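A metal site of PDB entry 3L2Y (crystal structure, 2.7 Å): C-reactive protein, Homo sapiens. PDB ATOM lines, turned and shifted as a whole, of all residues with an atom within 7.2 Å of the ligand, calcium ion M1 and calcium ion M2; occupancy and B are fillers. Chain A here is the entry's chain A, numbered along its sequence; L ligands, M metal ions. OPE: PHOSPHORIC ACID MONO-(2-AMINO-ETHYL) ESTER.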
ATOM      1  N   TYR A  49      -3.085  -7.127  21.512  1.00  0.00           N
ATOM      2  CA  TYR A  49      -2.733  -6.598  20.202  1.00  0.00           C
ATOM      3  C   TYR A  49      -3.945  -6.129  19.407  1.00  0.00           C
ATOM      4  O   TYR A  49      -5.064  -6.609  19.628  1.00  0.00           O
ATOM      5  CB  TYR A  49      -1.959  -7.619  19.367  1.00  0.00           C
ATOM      6  CG  TYR A  49      -2.639  -8.952  19.241  1.00  0.00           C
ATOM      7  CD1 TYR A  49      -3.476  -9.228  18.179  1.00  0.00           C
ATOM      8  CD2 TYR A  49      -2.415  -9.946  20.173  1.00  0.00           C
ATOM      9  CE1 TYR A  49      -4.091 -10.467  18.059  1.00  0.00           C
ATOM     10  CE2 TYR A  49      -3.020 -11.174  20.062  1.00  0.00           C
ATOM     11  CZ  TYR A  49      -3.868 -11.430  19.011  1.00  0.00           C
ATOM     12  OH  TYR A  49      -4.473 -12.668  18.920  1.00  0.00           O
ATOM     13  N   SER A  50      -3.715  -5.179  18.493  1.00  0.00           N
ATOM     14  CA  SER A  50      -4.762  -4.662  17.623  1.00  0.00           C
ATOM     15  C   SER A  50      -4.875  -5.471  16.330  1.00  0.00           C
ATOM     16  O   SER A  50      -3.892  -5.687  15.616  1.00  0.00           O
ATOM     17  CB  SER A  50      -4.515  -3.180  17.309  1.00  0.00           C
ATOM     18  OG  SER A  50      -5.263  -2.771  16.182  1.00  0.00           O
ATOM     19  N   SER A  53      -7.826  -1.471  13.291  1.00  0.00           N
ATOM     20  CA  SER A  53      -8.023  -0.150  13.903  1.00  0.00           C
ATOM     21  C   SER A  53      -8.601   0.883  12.940  1.00  0.00           C
ATOM     22  O   SER A  53      -7.988   1.212  11.926  1.00  0.00           O
ATOM     23  CB  SER A  53      -6.714   0.405  14.486  1.00  0.00           C
ATOM     24  OG  SER A  53      -6.944   1.635  15.160  1.00  0.00           O
ATOM     25  N   GLN A  59     -12.722  10.255  17.181  1.00  0.00           N
ATOM     26  CA  GLN A  59     -12.669   9.018  17.962  1.00  0.00           C
ATOM     27  C   GLN A  59     -11.599   8.069  17.429  1.00  0.00           C
ATOM     28  O   GLN A  59     -11.685   7.585  16.299  1.00  0.00           O
ATOM     29  CB  GLN A  59     -14.044   8.339  17.954  1.00  0.00           C
ATOM     30  CG  GLN A  59     -14.058   6.976  18.589  1.00  0.00           C
ATOM     31  CD  GLN A  59     -13.837   7.033  20.073  1.00  0.00           C
ATOM     32  OE1 GLN A  59     -12.824   6.568  20.582  1.00  0.00           O
ATOM     33  NE2 GLN A  59     -14.801   7.611  20.790  1.00  0.00           N
ATOM     34  N   ASP A  60     -10.587   7.799  18.255  1.00  0.00           N
ATOM     35  CA  ASP A  60      -9.497   6.913  17.860  1.00  0.00           C
ATOM     36  C   ASP A  60      -9.939   5.454  17.749  1.00  0.00           C
ATOM     37  O   ASP A  60      -9.367   4.683  16.996  1.00  0.00           O
ATOM     38  CB  ASP A  60      -8.305   7.067  18.813  1.00  0.00           C
ATOM     39  CG  ASP A  60      -8.643   6.721  20.270  1.00  0.00           C
ATOM     40  OD1 ASP A  60      -9.759   7.026  20.737  1.00  0.00           O
ATOM     41  OD2 ASP A  60      -7.770   6.161  20.956  1.00  0.00           O
ATOM     42  N   ASN A  61     -10.990   5.106  18.485  1.00  0.00           N
ATOM     43  CA  ASN A  61     -11.526   3.762  18.465  1.00  0.00           C
ATOM     44  C   ASN A  61     -12.933   3.723  17.915  1.00  0.00           C
ATOM     45  O   ASN A  61     -13.859   3.261  18.591  1.00  0.00           O
ATOM     46  CB  ASN A  61     -11.471   3.178  19.875  1.00  0.00           C
ATOM     47  CG  ASN A  61     -10.049   3.127  20.415  1.00  0.00           C
ATOM     48  OD1 ASN A  61      -9.108   3.490  19.721  1.00  0.00           O
ATOM     49  ND2 ASN A  61      -9.897   2.675  21.640  1.00  0.00           N
ATOM     50  N   LEU A  64     -12.894  -0.885  16.527  1.00  0.00           N
ATOM     51  CA  LEU A  64     -11.661  -1.549  16.954  1.00  0.00           C
ATOM     52  C   LEU A  64     -11.859  -3.018  17.286  1.00  0.00           C
ATOM     53  O   LEU A  64     -12.594  -3.365  18.204  1.00  0.00           O
ATOM     54  CB  LEU A  64     -11.025  -0.842  18.153  1.00  0.00           C
ATOM     55  CG  LEU A  64      -9.759  -1.534  18.640  1.00  0.00           C
ATOM     56  CD1 LEU A  64      -8.662  -1.458  17.587  1.00  0.00           C
ATOM     57  CD2 LEU A  64      -9.262  -0.953  19.956  1.00  0.00           C
ATOM     58  N   PHE A  66      -9.754  -6.030  18.691  1.00  0.00           N
ATOM     59  CA  PHE A  66      -8.554  -6.089  19.508  1.00  0.00           C
ATOM     60  C   PHE A  66      -8.537  -7.377  20.322  1.00  0.00           C
ATOM     61  O   PHE A  66      -9.589  -7.891  20.711  1.00  0.00           O
ATOM     62  CB  PHE A  66      -8.583  -4.903  20.448  1.00  0.00           C
ATOM     63  CG  PHE A  66      -7.320  -4.688  21.209  1.00  0.00           C
ATOM     64  CD1 PHE A  66      -6.329  -3.869  20.695  1.00  0.00           C
ATOM     65  CD2 PHE A  66      -7.141  -5.249  22.464  1.00  0.00           C
ATOM     66  CE1 PHE A  66      -5.159  -3.630  21.408  1.00  0.00           C
ATOM     67  CE2 PHE A  66      -5.971  -5.020  23.177  1.00  0.00           C
ATOM     68  CZ  PHE A  66      -4.990  -4.212  22.644  1.00  0.00           C
ATOM     69  N   TRP A  67      -7.357  -7.927  20.558  1.00  0.00           N
ATOM     70  CA  TRP A  67      -7.246  -9.078  21.436  1.00  0.00           C
ATOM     71  C   TRP A  67      -6.655  -8.582  22.731  1.00  0.00           C
ATOM     72  O   TRP A  67      -5.541  -8.058  22.750  1.00  0.00           O
ATOM     73  CB  TRP A  67      -6.322 -10.147  20.838  1.00  0.00           C
ATOM     74  CG  TRP A  67      -6.080 -11.259  21.812  1.00  0.00           C
ATOM     75  CD1 TRP A  67      -5.086 -11.328  22.756  1.00  0.00           C
ATOM     76  CD2 TRP A  67      -6.850 -12.443  21.966  1.00  0.00           C
ATOM     77  NE1 TRP A  67      -5.199 -12.494  23.480  1.00  0.00           N
ATOM     78  CE2 TRP A  67      -6.276 -13.194  23.013  1.00  0.00           C
ATOM     79  CE3 TRP A  67      -7.972 -12.958  21.317  1.00  0.00           C
ATOM     80  CZ2 TRP A  67      -6.786 -14.409  23.420  1.00  0.00           C
ATOM     81  CZ3 TRP A  67      -8.474 -14.162  21.723  1.00  0.00           C
ATOM     82  CH2 TRP A  67      -7.891 -14.883  22.770  1.00  0.00           C
ATOM     83  N   SER A  68      -7.396  -8.727  23.825  1.00  0.00           N
ATOM     84  CA  SER A  68      -6.850  -8.314  25.113  1.00  0.00           C
ATOM     85  C   SER A  68      -6.406  -9.527  25.953  1.00  0.00           C
ATOM     86  O   SER A  68      -7.118 -10.538  26.021  1.00  0.00           O
ATOM     87  CB  SER A  68      -7.803  -7.364  25.863  1.00  0.00           C
ATOM     88  OG  SER A  68      -8.900  -8.069  26.378  1.00  0.00           O
ATOM     89  N   SER A  74     -11.898  -8.202  21.993  1.00  0.00           N
ATOM     90  CA  SER A  74     -12.557  -6.970  22.400  1.00  0.00           C
ATOM     91  C   SER A  74     -13.046  -6.227  21.170  1.00  0.00           C
ATOM     92  O   SER A  74     -12.287  -5.969  20.233  1.00  0.00           O
ATOM     93  CB  SER A  74     -11.600  -6.101  23.208  1.00  0.00           C
ATOM     94  OG  SER A  74     -11.620  -4.768  22.724  1.00  0.00           O
ATOM     95  N   THR A  76     -14.895  -2.789  19.780  1.00  0.00           N
ATOM     96  CA  THR A  76     -15.221  -1.429  20.155  1.00  0.00           C
ATOM     97  C   THR A  76     -15.860  -0.643  19.008  1.00  0.00           C
ATOM     98  O   THR A  76     -15.344  -0.612  17.892  1.00  0.00           O
ATOM     99  CB  THR A  76     -13.966  -0.678  20.636  1.00  0.00           C
ATOM    100  OG1 THR A  76     -13.292  -1.455  21.641  1.00  0.00           O
ATOM    101  CG2 THR A  76     -14.347   0.681  21.193  1.00  0.00           C
ATOM    102  N   GLU A  81     -16.819  -0.497  24.486  1.00  0.00           N
ATOM    103  CA  GLU A  81     -16.218  -1.808  24.333  1.00  0.00           C
ATOM    104  C   GLU A  81     -17.123  -2.902  24.869  1.00  0.00           C
ATOM    105  O   GLU A  81     -17.732  -2.739  25.924  1.00  0.00           O
ATOM    106  CB  GLU A  81     -14.872  -1.839  25.075  1.00  0.00           C
ATOM    107  CG  GLU A  81     -14.118  -3.149  25.027  1.00  0.00           C
ATOM    108  CD  GLU A  81     -12.888  -3.165  25.923  1.00  0.00           C
ATOM    109  OE1 GLU A  81     -13.041  -2.843  27.122  1.00  0.00           O
ATOM    110  OE2 GLU A  81     -11.772  -3.480  25.437  1.00  0.00           O
ATOM    111  N   GLU A 138      -2.197  -0.024  16.666  1.00  0.00           N
ATOM    112  CA  GLU A 138      -3.429   0.467  17.262  1.00  0.00           C
ATOM    113  C   GLU A 138      -3.333   1.986  17.322  1.00  0.00           C
ATOM    114  O   GLU A 138      -2.367   2.541  17.845  1.00  0.00           O
ATOM    115  CB  GLU A 138      -3.636  -0.113  18.659  1.00  0.00           C
ATOM    116  CG  GLU A 138      -5.093  -0.138  19.152  1.00  0.00           C
ATOM    117  CD  GLU A 138      -5.643   1.249  19.463  1.00  0.00           C
ATOM    118  OE1 GLU A 138      -4.961   1.981  20.200  1.00  0.00           O
ATOM    119  OE2 GLU A 138      -6.740   1.609  18.957  1.00  0.00           O
ATOM    120  N   GLN A 139      -4.330   2.661  16.748  1.00  0.00           N
ATOM    121  CA  GLN A 139      -4.344   4.122  16.672  1.00  0.00           C
ATOM    122  C   GLN A 139      -4.845   4.775  17.945  1.00  0.00           C
ATOM    123  O   GLN A 139      -5.901   4.413  18.462  1.00  0.00           O
ATOM    124  CB  GLN A 139      -5.245   4.563  15.529  1.00  0.00           C
ATOM    125  CG  GLN A 139      -4.636   4.415  14.164  1.00  0.00           C
ATOM    126  CD  GLN A 139      -5.652   4.629  13.068  1.00  0.00           C
ATOM    127  OE1 GLN A 139      -5.528   5.565  12.267  1.00  0.00           O
ATOM    128  NE2 GLN A 139      -6.677   3.779  13.043  1.00  0.00           N
ATOM    129  N   ASP A 140      -4.093   5.748  18.447  1.00  0.00           N
ATOM    130  CA  ASP A 140      -4.568   6.570  19.546  1.00  0.00           C
ATOM    131  C   ASP A 140      -4.902   7.976  19.060  1.00  0.00           C
ATOM    132  O   ASP A 140      -5.438   8.799  19.791  1.00  0.00           O
ATOM    133  CB  ASP A 140      -3.527   6.638  20.656  1.00  0.00           C
ATOM    134  CG  ASP A 140      -3.593   5.447  21.570  1.00  0.00           C
ATOM    135  OD1 ASP A 140      -4.637   4.756  21.552  1.00  0.00           O
ATOM    136  OD2 ASP A 140      -2.625   5.204  22.317  1.00  0.00           O
ATOM    137  N   SER A 141      -4.584   8.244  17.795  1.00  0.00           N
ATOM    138  CA  SER A 141      -4.934   9.496  17.172  1.00  0.00           C
ATOM    139  C   SER A 141      -5.220   9.195  15.725  1.00  0.00           C
ATOM    140  O   SER A 141      -4.873   8.125  15.234  1.00  0.00           O
ATOM    141  CB  SER A 141      -3.784  10.495  17.292  1.00  0.00           C
ATOM    142  OG  SER A 141      -2.752  10.188  16.377  1.00  0.00           O
ATOM    143  N   GLY A 144      -2.168   7.843  13.691  1.00  0.00           N
ATOM    144  CA  GLY A 144      -0.926   7.705  14.419  1.00  0.00           C
ATOM    145  C   GLY A 144      -1.029   7.474  15.917  1.00  0.00           C
ATOM    146  O   GLY A 144      -2.059   7.003  16.435  1.00  0.00           O
ATOM    147  N   ASN A 145       0.054   7.817  16.610  1.00  0.00           N
ATOM    148  CA  ASN A 145       0.160   7.586  18.042  1.00  0.00           C
ATOM    149  C   ASN A 145       0.022   6.121  18.382  1.00  0.00           C
ATOM    150  O   ASN A 145      -0.865   5.733  19.145  1.00  0.00           O
ATOM    151  CB  ASN A 145      -0.845   8.413  18.826  1.00  0.00           C
ATOM    152  CG  ASN A 145      -0.335   9.799  19.097  1.00  0.00           C
ATOM    153  OD1 ASN A 145      -0.944  10.790  18.676  1.00  0.00           O
ATOM    154  ND2 ASN A 145       0.792   9.895  19.773  1.00  0.00           N
ATOM    155  N   PHE A 146       0.913   5.321  17.821  1.00  0.00           N
ATOM    156  CA  PHE A 146       0.889   3.880  17.998  1.00  0.00           C
ATOM    157  C   PHE A 146       1.581   3.490  19.296  1.00  0.00           C
ATOM    158  O   PHE A 146       2.466   4.200  19.758  1.00  0.00           O
ATOM    159  CB  PHE A 146       1.593   3.220  16.819  1.00  0.00           C
ATOM    160  CG  PHE A 146       1.086   3.690  15.484  1.00  0.00           C
ATOM    161  CD1 PHE A 146      -0.276   3.708  15.213  1.00  0.00           C
ATOM    162  CD2 PHE A 146       1.954   4.124  14.501  1.00  0.00           C
ATOM    163  CE1 PHE A 146      -0.738   4.143  13.987  1.00  0.00           C
ATOM    164  CE2 PHE A 146       1.493   4.549  13.276  1.00  0.00           C
ATOM    165  CZ  PHE A 146       0.142   4.558  13.014  1.00  0.00           C
ATOM    166  N   GLU A 147       1.160   2.374  19.888  1.00  0.00           N
ATOM    167  CA  GLU A 147       1.848   1.791  21.030  1.00  0.00           C
ATOM    168  C   GLU A 147       2.402   0.453  20.598  1.00  0.00           C
ATOM    169  O   GLU A 147       1.682  -0.388  20.053  1.00  0.00           O
ATOM    170  CB  GLU A 147       0.903   1.577  22.221  1.00  0.00           C
ATOM    171  CG  GLU A 147       0.209   2.809  22.789  1.00  0.00           C
ATOM    172  CD  GLU A 147      -0.516   2.519  24.116  1.00  0.00           C
ATOM    173  OE1 GLU A 147       0.174   2.153  25.093  1.00  0.00           O
ATOM    174  OE2 GLU A 147      -1.764   2.649  24.189  1.00  0.00           O
ATOM    175  N   GLN A 150       1.017  -2.895  21.588  1.00  0.00           N
ATOM    176  CA  GLN A 150      -0.283  -3.239  21.021  1.00  0.00           C
ATOM    177  C   GLN A 150      -0.196  -3.599  19.545  1.00  0.00           C
ATOM    178  O   GLN A 150      -1.217  -3.798  18.887  1.00  0.00           O
ATOM    179  CB  GLN A 150      -1.274  -2.090  21.229  1.00  0.00           C
ATOM    180  CG  GLN A 150      -1.662  -1.908  22.678  1.00  0.00           C
ATOM    181  CD  GLN A 150      -2.699  -0.832  22.858  1.00  0.00           C
ATOM    182  OE1 GLN A 150      -2.754   0.083  22.063  1.00  0.00           O
ATOM    183  NE2 GLN A 150      -3.534  -0.953  23.885  1.00  0.00           N
HETATM  184  CA  OPE L   1      -7.786  -0.153  23.261  1.00  0.00           C
HETATM  185  CB  OPE L   1      -7.920  -1.632  23.372  1.00  0.00           C
HETATM  186  O1  OPE L   1      -7.333   2.507  22.640  1.00  0.00           O
HETATM  187  O2  OPE L   1      -5.101   2.416  23.408  1.00  0.00           O
HETATM  188  O3  OPE L   1      -6.970   2.647  25.029  1.00  0.00           O
HETATM  189  O4  OPE L   1      -6.594   0.464  23.746  1.00  0.00           O
HETATM  190  N   OPE L   1      -8.453  -2.182  24.628  1.00  0.00           N
HETATM  191  P   OPE L   1      -6.502   2.042  23.765  1.00  0.00           P
HETATM  192 CA    CA M   1      -6.818   3.685  20.613  1.00  0.00          CA
HETATM  193 CA    CA M   2      -3.301   2.667  22.052  1.00  0.00          CA
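OE2 of Glu 81 is in salt-bridge range of N of the ligand, 3.7 Å away.
OG of Ser 53 lies within hydrogen-bond range of NE2 of Gln 139.
N of Asn 61 is in hydrogen-bond range of OE1 of Gln 59, 3.1 Å away.
The backbone NH of Asp 140 sits close to the backbone carbonyl oxygen of Asn 145.
The backbone carbonyl oxygen (O) of Gln 150 sits at hydrogen-bond distance from the backbone NH (N) of Ser 50 (2.9 Å).
The side-chain carboxylate (OD1) of Asp 60 lies close to the side-chain amide oxygen (OE1) of Gln 59, 3.1 Å away.
The side-chain carboxylate (OE2) of Glu 81 is in hydrogen-bond range of the side-chain hydroxyl (OG) of Ser 74 (3.0 Å).
The backbone NH (N) of Leu 64 lies within hydrogen-bond range of the backbone carbonyl oxygen (O) of Thr 76.
The backbone carbonyl oxygen (O) of Phe 66 sits at hydrogen-bond distance from the backbone NH (N) of Ser 74 (2.7 Å).
Leu 64 touches the ligand.
Phe 66 touches the ligand (CG to CB, 3.8 Å).
Hydrophobic or aromatic side chains that line the ligand: Leu 64 and Phe 66.
Eight residues have an atom within 4 Å of the ligand: Asn 61, Leu 64, Phe 66, Glu 81, Glu 138, Asp 140, Glu 147 and Gln 150.
The nearest printed residue that does not touch calcium ion M1 is Leu 64 (5.3 Å).
Calcium ion M1 is bound by O1 of the ligand, O of Gln 139, OD1 of Asn 61, OE1 of Glu 138, OD1 of Asp 140, OE2 of Glu 138 and OD2 of Asp 60.
Calcium ion M1 has seven donor atoms within binding distance.
Calcium ion M2 is bound by O2 of the ligand, OD1 of Asp 140, OE1 of Glu 138, OE2 of Glu 147, OD2 of Asp 140 and OE1 of Gln 150.
Calcium ion M2 has six donor atoms within binding distance.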
